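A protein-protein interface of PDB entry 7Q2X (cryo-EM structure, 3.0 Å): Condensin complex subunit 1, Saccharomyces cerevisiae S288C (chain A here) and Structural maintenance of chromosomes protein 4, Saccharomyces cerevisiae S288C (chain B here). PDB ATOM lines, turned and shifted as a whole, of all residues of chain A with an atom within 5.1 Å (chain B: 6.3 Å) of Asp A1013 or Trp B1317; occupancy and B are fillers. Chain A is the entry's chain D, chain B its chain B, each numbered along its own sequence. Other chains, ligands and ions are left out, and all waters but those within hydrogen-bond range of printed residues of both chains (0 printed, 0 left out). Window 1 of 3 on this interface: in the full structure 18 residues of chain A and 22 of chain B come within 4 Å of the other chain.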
ATOM      1  N   ASN A1009      -3.428  -5.038 -12.038  1.00  0.00           N
ATOM      2  CA  ASN A1009      -2.422  -4.761 -11.020  1.00  0.00           C
ATOM      3  C   ASN A1009      -2.266  -3.272 -10.738  1.00  0.00           C
ATOM      4  O   ASN A1009      -1.691  -2.905  -9.709  1.00  0.00           O
ATOM      5  CB  ASN A1009      -1.078  -5.355 -11.445  1.00  0.00           C
ATOM      6  CG  ASN A1009      -0.127  -5.546 -10.280  1.00  0.00           C
ATOM      7  OD1 ASN A1009      -0.477  -5.291  -9.128  1.00  0.00           O
ATOM      8  ND2 ASN A1009       1.083  -6.004 -10.575  1.00  0.00           N
ATOM      9  N   ASN A1010      -2.769  -2.410 -11.623  1.00  0.00           N
ATOM     10  CA  ASN A1010      -2.639  -0.972 -11.412  1.00  0.00           C
ATOM     11  C   ASN A1010      -3.379  -0.524 -10.157  1.00  0.00           C
ATOM     12  O   ASN A1010      -2.878   0.314  -9.399  1.00  0.00           O
ATOM     13  CB  ASN A1010      -3.148  -0.221 -12.640  1.00  0.00           C
ATOM     14  CG  ASN A1010      -2.622  -0.807 -13.939  1.00  0.00           C
ATOM     15  OD1 ASN A1010      -2.956  -1.933 -14.307  1.00  0.00           O
ATOM     16  ND2 ASN A1010      -1.791  -0.042 -14.637  1.00  0.00           N
ATOM     17  N   LEU A1011      -4.570  -1.071  -9.919  1.00  0.00           N
ATOM     18  CA  LEU A1011      -5.385  -0.631  -8.795  1.00  0.00           C
ATOM     19  C   LEU A1011      -4.914  -1.199  -7.460  1.00  0.00           C
ATOM     20  O   LEU A1011      -5.290  -0.666  -6.410  1.00  0.00           O
ATOM     21  CB  LEU A1011      -6.844  -1.024  -9.032  1.00  0.00           C
ATOM     22  CG  LEU A1011      -7.523  -0.327 -10.213  1.00  0.00           C
ATOM     23  CD1 LEU A1011      -8.919  -0.888 -10.442  1.00  0.00           C
ATOM     24  CD2 LEU A1011      -7.555   1.183 -10.043  1.00  0.00           C
ATOM     25  N   VAL A1012      -4.111  -2.262  -7.474  1.00  0.00           N
ATOM     26  CA  VAL A1012      -3.715  -2.962  -6.255  1.00  0.00           C
ATOM     27  C   VAL A1012      -2.221  -2.825  -5.968  1.00  0.00           C
ATOM     28  O   VAL A1012      -1.772  -3.209  -4.873  1.00  0.00           O
ATOM     29  CB  VAL A1012      -4.131  -4.451  -6.319  1.00  0.00           C
ATOM     30  CG1 VAL A1012      -3.798  -5.229  -5.039  1.00  0.00           C
ATOM     31  CG2 VAL A1012      -5.615  -4.563  -6.639  1.00  0.00           C
ATOM     32  N   ASP A1013      -1.441  -2.263  -6.894  1.00  0.00           N
ATOM     33  CA  ASP A1013      -0.004  -2.134  -6.673  1.00  0.00           C
ATOM     34  C   ASP A1013       0.296  -1.272  -5.452  1.00  0.00           C
ATOM     35  O   ASP A1013       1.202  -1.583  -4.670  1.00  0.00           O
ATOM     36  CB  ASP A1013       0.667  -1.555  -7.918  1.00  0.00           C
ATOM     37  CG  ASP A1013       2.157  -1.824  -7.953  1.00  0.00           C
ATOM     38  OD1 ASP A1013       2.621  -2.689  -7.181  1.00  0.00           O
ATOM     39  OD2 ASP A1013       2.865  -1.171  -8.749  1.00  0.00           O
ATOM     40  N   GLU A1014      -0.453  -0.182  -5.272  1.00  0.00           N
ATOM     41  CA  GLU A1014      -0.209   0.701  -4.136  1.00  0.00           C
ATOM     42  C   GLU A1014      -0.690   0.090  -2.825  1.00  0.00           C
ATOM     43  O   GLU A1014      -0.071   0.312  -1.778  1.00  0.00           O
ATOM     44  CB  GLU A1014      -0.883   2.055  -4.366  1.00  0.00           C
ATOM     45  CG  GLU A1014      -0.286   2.874  -5.503  1.00  0.00           C
ATOM     46  CD  GLU A1014      -0.820   2.471  -6.866  1.00  0.00           C
ATOM     47  OE1 GLU A1014      -1.705   1.592  -6.926  1.00  0.00           O
ATOM     48  OE2 GLU A1014      -0.354   3.035  -7.878  1.00  0.00           O
ATOM     49  N   ASN A1015      -1.779  -0.675  -2.857  1.00  0.00           N
ATOM     50  CA  ASN A1015      -2.376  -1.239  -1.653  1.00  0.00           C
ATOM     51  C   ASN A1015      -1.864  -2.638  -1.333  1.00  0.00           C
ATOM     52  O   ASN A1015      -2.364  -3.266  -0.395  1.00  0.00           O
ATOM     53  CB  ASN A1015      -3.901  -1.264  -1.785  1.00  0.00           C
ATOM     54  CG  ASN A1015      -4.468   0.074  -2.213  1.00  0.00           C
ATOM     55  OD1 ASN A1015      -4.556   1.008  -1.415  1.00  0.00           O
ATOM     56  ND2 ASN A1015      -4.857   0.174  -3.478  1.00  0.00           N
ATOM     57  N   THR A1016      -0.892  -3.141  -2.100  1.00  0.00           N
ATOM     58  CA  THR A1016      -0.302  -4.444  -1.805  1.00  0.00           C
ATOM     59  C   THR A1016       0.241  -4.521  -0.381  1.00  0.00           C
ATOM     60  O   THR A1016       0.248  -5.600   0.225  1.00  0.00           O
ATOM     61  CB  THR A1016       0.807  -4.746  -2.818  1.00  0.00           C
ATOM     62  OG1 THR A1016       0.253  -4.760  -4.139  1.00  0.00           O
ATOM     63  CG2 THR A1016       1.449  -6.098  -2.543  1.00  0.00           C
ATOM     64  N   GLY A1045       6.521 -12.521 -10.179  1.00  0.00           N
ATOM     65  CA  GLY A1045       7.011 -11.206 -10.534  1.00  0.00           C
ATOM     66  C   GLY A1045       5.981 -10.102 -10.492  1.00  0.00           C
ATOM     67  O   GLY A1045       6.294  -8.971 -10.879  1.00  0.00           O
ATOM     68  N   GLN A1046       4.761 -10.393 -10.037  1.00  0.00           N
ATOM     69  CA  GLN A1046       3.717  -9.373 -10.008  1.00  0.00           C
ATOM     70  C   GLN A1046       3.995  -8.320  -8.942  1.00  0.00           C
ATOM     71  O   GLN A1046       3.698  -7.136  -9.140  1.00  0.00           O
ATOM     72  CB  GLN A1046       2.356 -10.026  -9.774  1.00  0.00           C
ATOM     73  CG  GLN A1046       2.059 -11.198 -10.696  1.00  0.00           C
ATOM     74  CD  GLN A1046       2.061 -10.805 -12.159  1.00  0.00           C
ATOM     75  OE1 GLN A1046       2.730 -11.431 -12.981  1.00  0.00           O
ATOM     76  NE2 GLN A1046       1.308  -9.764 -12.493  1.00  0.00           N
ATOM     77  N   VAL A1047       4.561  -8.726  -7.809  1.00  0.00           N
ATOM     78  CA  VAL A1047       4.784  -7.844  -6.670  1.00  0.00           C
ATOM     79  C   VAL A1047       6.268  -7.856  -6.328  1.00  0.00           C
ATOM     80  O   VAL A1047       6.874  -8.927  -6.210  1.00  0.00           O
ATOM     81  CB  VAL A1047       3.937  -8.265  -5.455  1.00  0.00           C
ATOM     82  CG1 VAL A1047       4.390  -7.527  -4.206  1.00  0.00           C
ATOM     83  CG2 VAL A1047       2.462  -8.012  -5.725  1.00  0.00           C
ATOM     84  N   LYS A1048       6.847  -6.668  -6.170  1.00  0.00           N
ATOM     85  CA  LYS A1048       8.253  -6.540  -5.826  1.00  0.00           C
ATOM     86  C   LYS A1048       8.477  -6.828  -4.343  1.00  0.00           C
ATOM     87  O   LYS A1048       7.542  -6.861  -3.538  1.00  0.00           O
ATOM     88  CB  LYS A1048       8.766  -5.144  -6.180  1.00  0.00           C
ATOM     89  CG  LYS A1048       8.480  -4.731  -7.614  1.00  0.00           C
ATOM     90  CD  LYS A1048       8.520  -3.222  -7.778  1.00  0.00           C
ATOM     91  CE  LYS A1048       9.914  -2.679  -7.518  1.00  0.00           C
ATOM     92  NZ  LYS A1048      10.875  -3.088  -8.580  1.00  0.00           N
ATOM     93  N   LYS B1279       3.964   6.913 -13.984  1.00  0.00           N
ATOM     94  CA  LYS B1279       3.132   5.716 -14.004  1.00  0.00           C
ATOM     95  C   LYS B1279       1.900   5.929 -14.874  1.00  0.00           C
ATOM     96  O   LYS B1279       1.546   5.070 -15.691  1.00  0.00           O
ATOM     97  CB  LYS B1279       2.731   5.336 -12.579  1.00  0.00           C
ATOM     98  CG  LYS B1279       1.967   4.026 -12.475  1.00  0.00           C
ATOM     99  CD  LYS B1279       1.545   3.749 -11.041  1.00  0.00           C
ATOM    100  CE  LYS B1279       2.731   3.328 -10.188  1.00  0.00           C
ATOM    101  NZ  LYS B1279       2.317   2.940  -8.812  1.00  0.00           N
ATOM    102  N   ASN B1290       3.511  -0.995 -15.692  1.00  0.00           N
ATOM    103  CA  ASN B1290       3.710   0.044 -14.695  1.00  0.00           C
ATOM    104  C   ASN B1290       5.115   0.618 -14.819  1.00  0.00           C
ATOM    105  O   ASN B1290       6.033  -0.046 -15.303  1.00  0.00           O
ATOM    106  CB  ASN B1290       3.493  -0.492 -13.273  1.00  0.00           C
ATOM    107  CG  ASN B1290       2.042  -0.817 -12.989  1.00  0.00           C
ATOM    108  OD1 ASN B1290       1.140  -0.070 -13.367  1.00  0.00           O
ATOM    109  ND2 ASN B1290       1.807  -1.938 -12.317  1.00  0.00           N
ATOM    110  N   ALA B1291       5.270   1.862 -14.380  1.00  0.00           N
ATOM    111  CA  ALA B1291       6.570   2.515 -14.314  1.00  0.00           C
ATOM    112  C   ALA B1291       6.759   3.062 -12.910  1.00  0.00           C
ATOM    113  O   ALA B1291       5.991   3.926 -12.471  1.00  0.00           O
ATOM    114  CB  ALA B1291       6.686   3.637 -15.350  1.00  0.00           C
ATOM    115  N   GLU B1292       7.773   2.565 -12.207  1.00  0.00           N
ATOM    116  CA  GLU B1292       7.978   2.908 -10.807  1.00  0.00           C
ATOM    117  C   GLU B1292       9.373   3.479 -10.607  1.00  0.00           C
ATOM    118  O   GLU B1292      10.360   2.890 -11.055  1.00  0.00           O
ATOM    119  CB  GLU B1292       7.777   1.685  -9.906  1.00  0.00           C
ATOM    120  CG  GLU B1292       7.930   1.969  -8.419  1.00  0.00           C
ATOM    121  CD  GLU B1292       6.863   2.906  -7.884  1.00  0.00           C
ATOM    122  OE1 GLU B1292       5.762   2.960  -8.472  1.00  0.00           O
ATOM    123  OE2 GLU B1292       7.126   3.592  -6.874  1.00  0.00           O
ATOM    124  N   SER B1309      12.023   1.074 -12.544  1.00  0.00           N
ATOM    125  CA  SER B1309      11.565  -0.270 -12.863  1.00  0.00           C
ATOM    126  C   SER B1309      10.358  -0.195 -13.788  1.00  0.00           C
ATOM    127  O   SER B1309       9.494   0.676 -13.632  1.00  0.00           O
ATOM    128  CB  SER B1309      11.205  -1.050 -11.595  1.00  0.00           C
ATOM    129  OG  SER B1309      12.346  -1.249 -10.778  1.00  0.00           O
ATOM    130  N   VAL B1310      10.309  -1.113 -14.751  1.00  0.00           N
ATOM    131  CA  VAL B1310       9.261  -1.149 -15.762  1.00  0.00           C
ATOM    132  C   VAL B1310       8.636  -2.536 -15.768  1.00  0.00           C
ATOM    133  O   VAL B1310       9.347  -3.544 -15.845  1.00  0.00           O
ATOM    134  CB  VAL B1310       9.807  -0.797 -17.160  1.00  0.00           C
ATOM    135  CG1 VAL B1310       8.858  -1.283 -18.241  1.00  0.00           C
ATOM    136  CG2 VAL B1310      10.030   0.699 -17.277  1.00  0.00           C
ATOM    137  N   MET B1311       7.310  -2.584 -15.687  1.00  0.00           N
ATOM    138  CA  MET B1311       6.552  -3.823 -15.801  1.00  0.00           C
ATOM    139  C   MET B1311       5.796  -3.812 -17.121  1.00  0.00           C
ATOM    140  O   MET B1311       4.779  -3.109 -17.238  1.00  0.00           O
ATOM    141  CB  MET B1311       5.583  -3.967 -14.628  1.00  0.00           C
ATOM    142  CG  MET B1311       4.797  -5.267 -14.609  1.00  0.00           C
ATOM    143  SD  MET B1311       3.752  -5.389 -13.145  1.00  0.00           S
ATOM    144  CE  MET B1311       2.897  -6.930 -13.458  1.00  0.00           C
ATOM    145  N   PRO B1312       6.244  -4.549 -18.132  1.00  0.00           N
ATOM    146  CA  PRO B1312       5.552  -4.547 -19.426  1.00  0.00           C
ATOM    147  C   PRO B1312       4.187  -5.200 -19.313  1.00  0.00           C
ATOM    148  O   PRO B1312       3.958  -6.026 -18.416  1.00  0.00           O
ATOM    149  CB  PRO B1312       6.490  -5.362 -20.332  1.00  0.00           C
ATOM    150  CG  PRO B1312       7.809  -5.378 -19.622  1.00  0.00           C
ATOM    151  CD  PRO B1312       7.478  -5.350 -18.166  1.00  0.00           C
ATOM    152  N   LYS B1315       3.286  -9.043 -18.453  1.00  0.00           N
ATOM    153  CA  LYS B1315       4.650  -9.438 -18.138  1.00  0.00           C
ATOM    154  C   LYS B1315       4.950  -9.071 -16.693  1.00  0.00           C
ATOM    155  O   LYS B1315       4.276  -8.232 -16.092  1.00  0.00           O
ATOM    156  CB  LYS B1315       5.663  -8.774 -19.080  1.00  0.00           C
ATOM    157  CG  LYS B1315       5.876  -9.511 -20.393  1.00  0.00           C
ATOM    158  CD  LYS B1315       7.072  -8.956 -21.148  1.00  0.00           C
ATOM    159  CE  LYS B1315       6.902  -9.118 -22.649  1.00  0.00           C
ATOM    160  NZ  LYS B1315       6.303  -7.907 -23.275  1.00  0.00           N
ATOM    161  N   SER B1316       5.976  -9.712 -16.142  1.00  0.00           N
ATOM    162  CA  SER B1316       6.372  -9.495 -14.761  1.00  0.00           C
ATOM    163  C   SER B1316       7.257  -8.255 -14.648  1.00  0.00           C
ATOM    164  O   SER B1316       7.605  -7.612 -15.642  1.00  0.00           O
ATOM    165  CB  SER B1316       7.086 -10.730 -14.214  1.00  0.00           C
ATOM    166  OG  SER B1316       8.376 -10.868 -14.784  1.00  0.00           O
ATOM    167  N   TRP B1317       7.617  -7.909 -13.415  1.00  0.00           N
ATOM    168  CA  TRP B1317       8.504  -6.777 -13.182  1.00  0.00           C
ATOM    169  C   TRP B1317       9.909  -7.097 -13.677  1.00  0.00           C
ATOM    170  O   TRP B1317      10.487  -8.132 -13.331  1.00  0.00           O
ATOM    171  CB  TRP B1317       8.540  -6.433 -11.693  1.00  0.00           C
ATOM    172  CG  TRP B1317       7.444  -5.511 -11.254  1.00  0.00           C
ATOM    173  CD1 TRP B1317       6.347  -5.839 -10.512  1.00  0.00           C
ATOM    174  CD2 TRP B1317       7.345  -4.106 -11.513  1.00  0.00           C
ATOM    175  NE1 TRP B1317       5.567  -4.728 -10.301  1.00  0.00           N
ATOM    176  CE2 TRP B1317       6.159  -3.651 -10.906  1.00  0.00           C
ATOM    177  CE3 TRP B1317       8.142  -3.188 -12.205  1.00  0.00           C
ATOM    178  CZ2 TRP B1317       5.750  -2.321 -10.967  1.00  0.00           C
ATOM    179  CZ3 TRP B1317       7.735  -1.869 -12.266  1.00  0.00           C
ATOM    180  CH2 TRP B1317       6.550  -1.448 -11.650  1.00  0.00           C
ATOM    181  N   ARG B1318      10.461  -6.200 -14.492  1.00  0.00           N
ATOM    182  CA  ARG B1318      11.793  -6.382 -15.050  1.00  0.00           C
ATOM    183  C   ARG B1318      12.565  -5.076 -14.963  1.00  0.00           C
ATOM    184  O   ARG B1318      11.987  -3.988 -14.908  1.00  0.00           O
ATOM    185  CB  ARG B1318      11.746  -6.859 -16.511  1.00  0.00           C
ATOM    186  CG  ARG B1318      10.613  -7.817 -16.830  1.00  0.00           C
ATOM    187  CD  ARG B1318      11.012  -8.789 -17.922  1.00  0.00           C
ATOM    188  NE  ARG B1318      12.290  -9.423 -17.622  1.00  0.00           N
ATOM    189  CZ  ARG B1318      12.423 -10.557 -16.949  1.00  0.00           C
ATOM    190  NH1 ARG B1318      11.372 -11.206 -16.472  1.00  0.00           N
ATOM    191  NH2 ARG B1318      13.641 -11.049 -16.741  1.00  0.00           N
ATOM    192  N   ASN B1319      13.889  -5.197 -14.943  1.00  0.00           N
ATOM    193  CA  ASN B1319      14.748  -4.027 -14.979  1.00  0.00           C
ATOM    194  C   ASN B1319      14.932  -3.546 -16.415  1.00  0.00           C
ATOM    195  O   ASN B1319      14.564  -4.222 -17.379  1.00  0.00           O
ATOM    196  CB  ASN B1319      16.102  -4.326 -14.333  1.00  0.00           C
ATOM    197  CG  ASN B1319      16.760  -5.568 -14.898  1.00  0.00           C
ATOM    198  OD1 ASN B1319      16.251  -6.184 -15.833  1.00  0.00           O
ATOM    199  ND2 ASN B1319      17.900  -5.944 -14.331  1.00  0.00           N
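The backbone carbonyl oxygen (O) of Asn B1290 sits at hydrogen-bond distance from the backbone NH (N) of Met B1311, 2.9 Å away.
N of Ser B1309 lies within hydrogen-bond range of O of Glu B1292 (2.9 Å).
The side-chain sulfur of Met B1311 lies within hydrogen-bond range of the indole nitrogen of Trp B1317 (3.4 Å).
OG of Ser B1316 lies within hydrogen-bond range of NH1 of Arg B1318 (3.5 Å).
O of Gln A1046 is in hydrogen-bond range of ND2 of Asn A1009 (3.2 Å).
The backbone carbonyl oxygen (O) of Asp A1013 sits at hydrogen-bond distance from the side-chain hydroxyl (OG1) of Thr A1016.
OD2 of Asp A1013 touches ND2 of Asn B1290 (3.8 Å).
CZ2 of Trp B1317 touches OD2 of Asp A1013, at 3.8 Å.
Gly A1045 touches Ser B1316 (CA to CB, 3.7 Å).
NE2 of Gln A1046 touches CE of Met B1311, 3.4 Å away.
Lys A1048 touches Trp B1317.
The side-chain amino group (NZ) of Lys B1279 is in salt-bridge range of the side-chain carboxylate (OE2) of Glu A1014 (2.8 Å).
The side-chain amide oxygen (OD1) of Asn B1290 is in hydrogen-bond range of the side-chain amide nitrogen (ND2) of Asn A1010, 3.2 Å away.
OG of Ser B1309 sits at hydrogen-bond distance from NZ of Lys A1048, 3.2 Å away.
ND2 of Asn A1009 sits close to SD of Met B1311, 3.8 Å away.
N of Trp B1317 sits at hydrogen-bond distance from O of Gly A1045 (3.1 Å).
The indole nitrogen (NE1) of Trp B1317 lies close to the backbone carbonyl oxygen (O) of Gln A1046.
Of the 12 printed residues of chain A, 7 touch a printed residue of chain B.
Printed residues of chain B that touch a printed residue of chain A: Lys B1279, Asn B1290, Ser B1309, Met B1311, Ser B1316 and Trp B1317.
Among the printed residues, 11 pairs touch across the chains.
Among the printed residues, Asp or Glu carboxylates within 4 Å of a Lys or Arg side-chain nitrogen of the other chain: Glu A1014 with Lys B1279 (2.8 Å).
Leu A1011 touches none of the printed residues of chain B.
Asp A1013 touches just these residues of chain B: Asn B1290 and Trp B1317.
Printed residues of chain B within 4 Å of Glu A1014: Lys B1279 (2.8 Å).
Of the printed residues of chain B, Gln A1046 touches Met B1311 and Trp B1317.
Glu B1292 touches none of the printed residues of chain A.
Of the printed residues of chain A, Ser B1309 touches Lys A1048 (3.2 Å).
Of chain A, only Asp A1013 (3.8 Å), Gly A1045 (3.1 Å), Gln A1046 (3.3 Å) and Lys A1048 (3.8 Å) come within 4 Å of Trp B1317.
The nearest residue of chain B that does not touch Asp A1013 is Lys B1279 (4.1 Å).
The nearest residue of chain A that does not touch Trp B1317 is Val A1047 (4.3 Å).
The nearest printed residue of chain B that does not touch Glu A1014 is Glu B1292 (6.1 Å).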
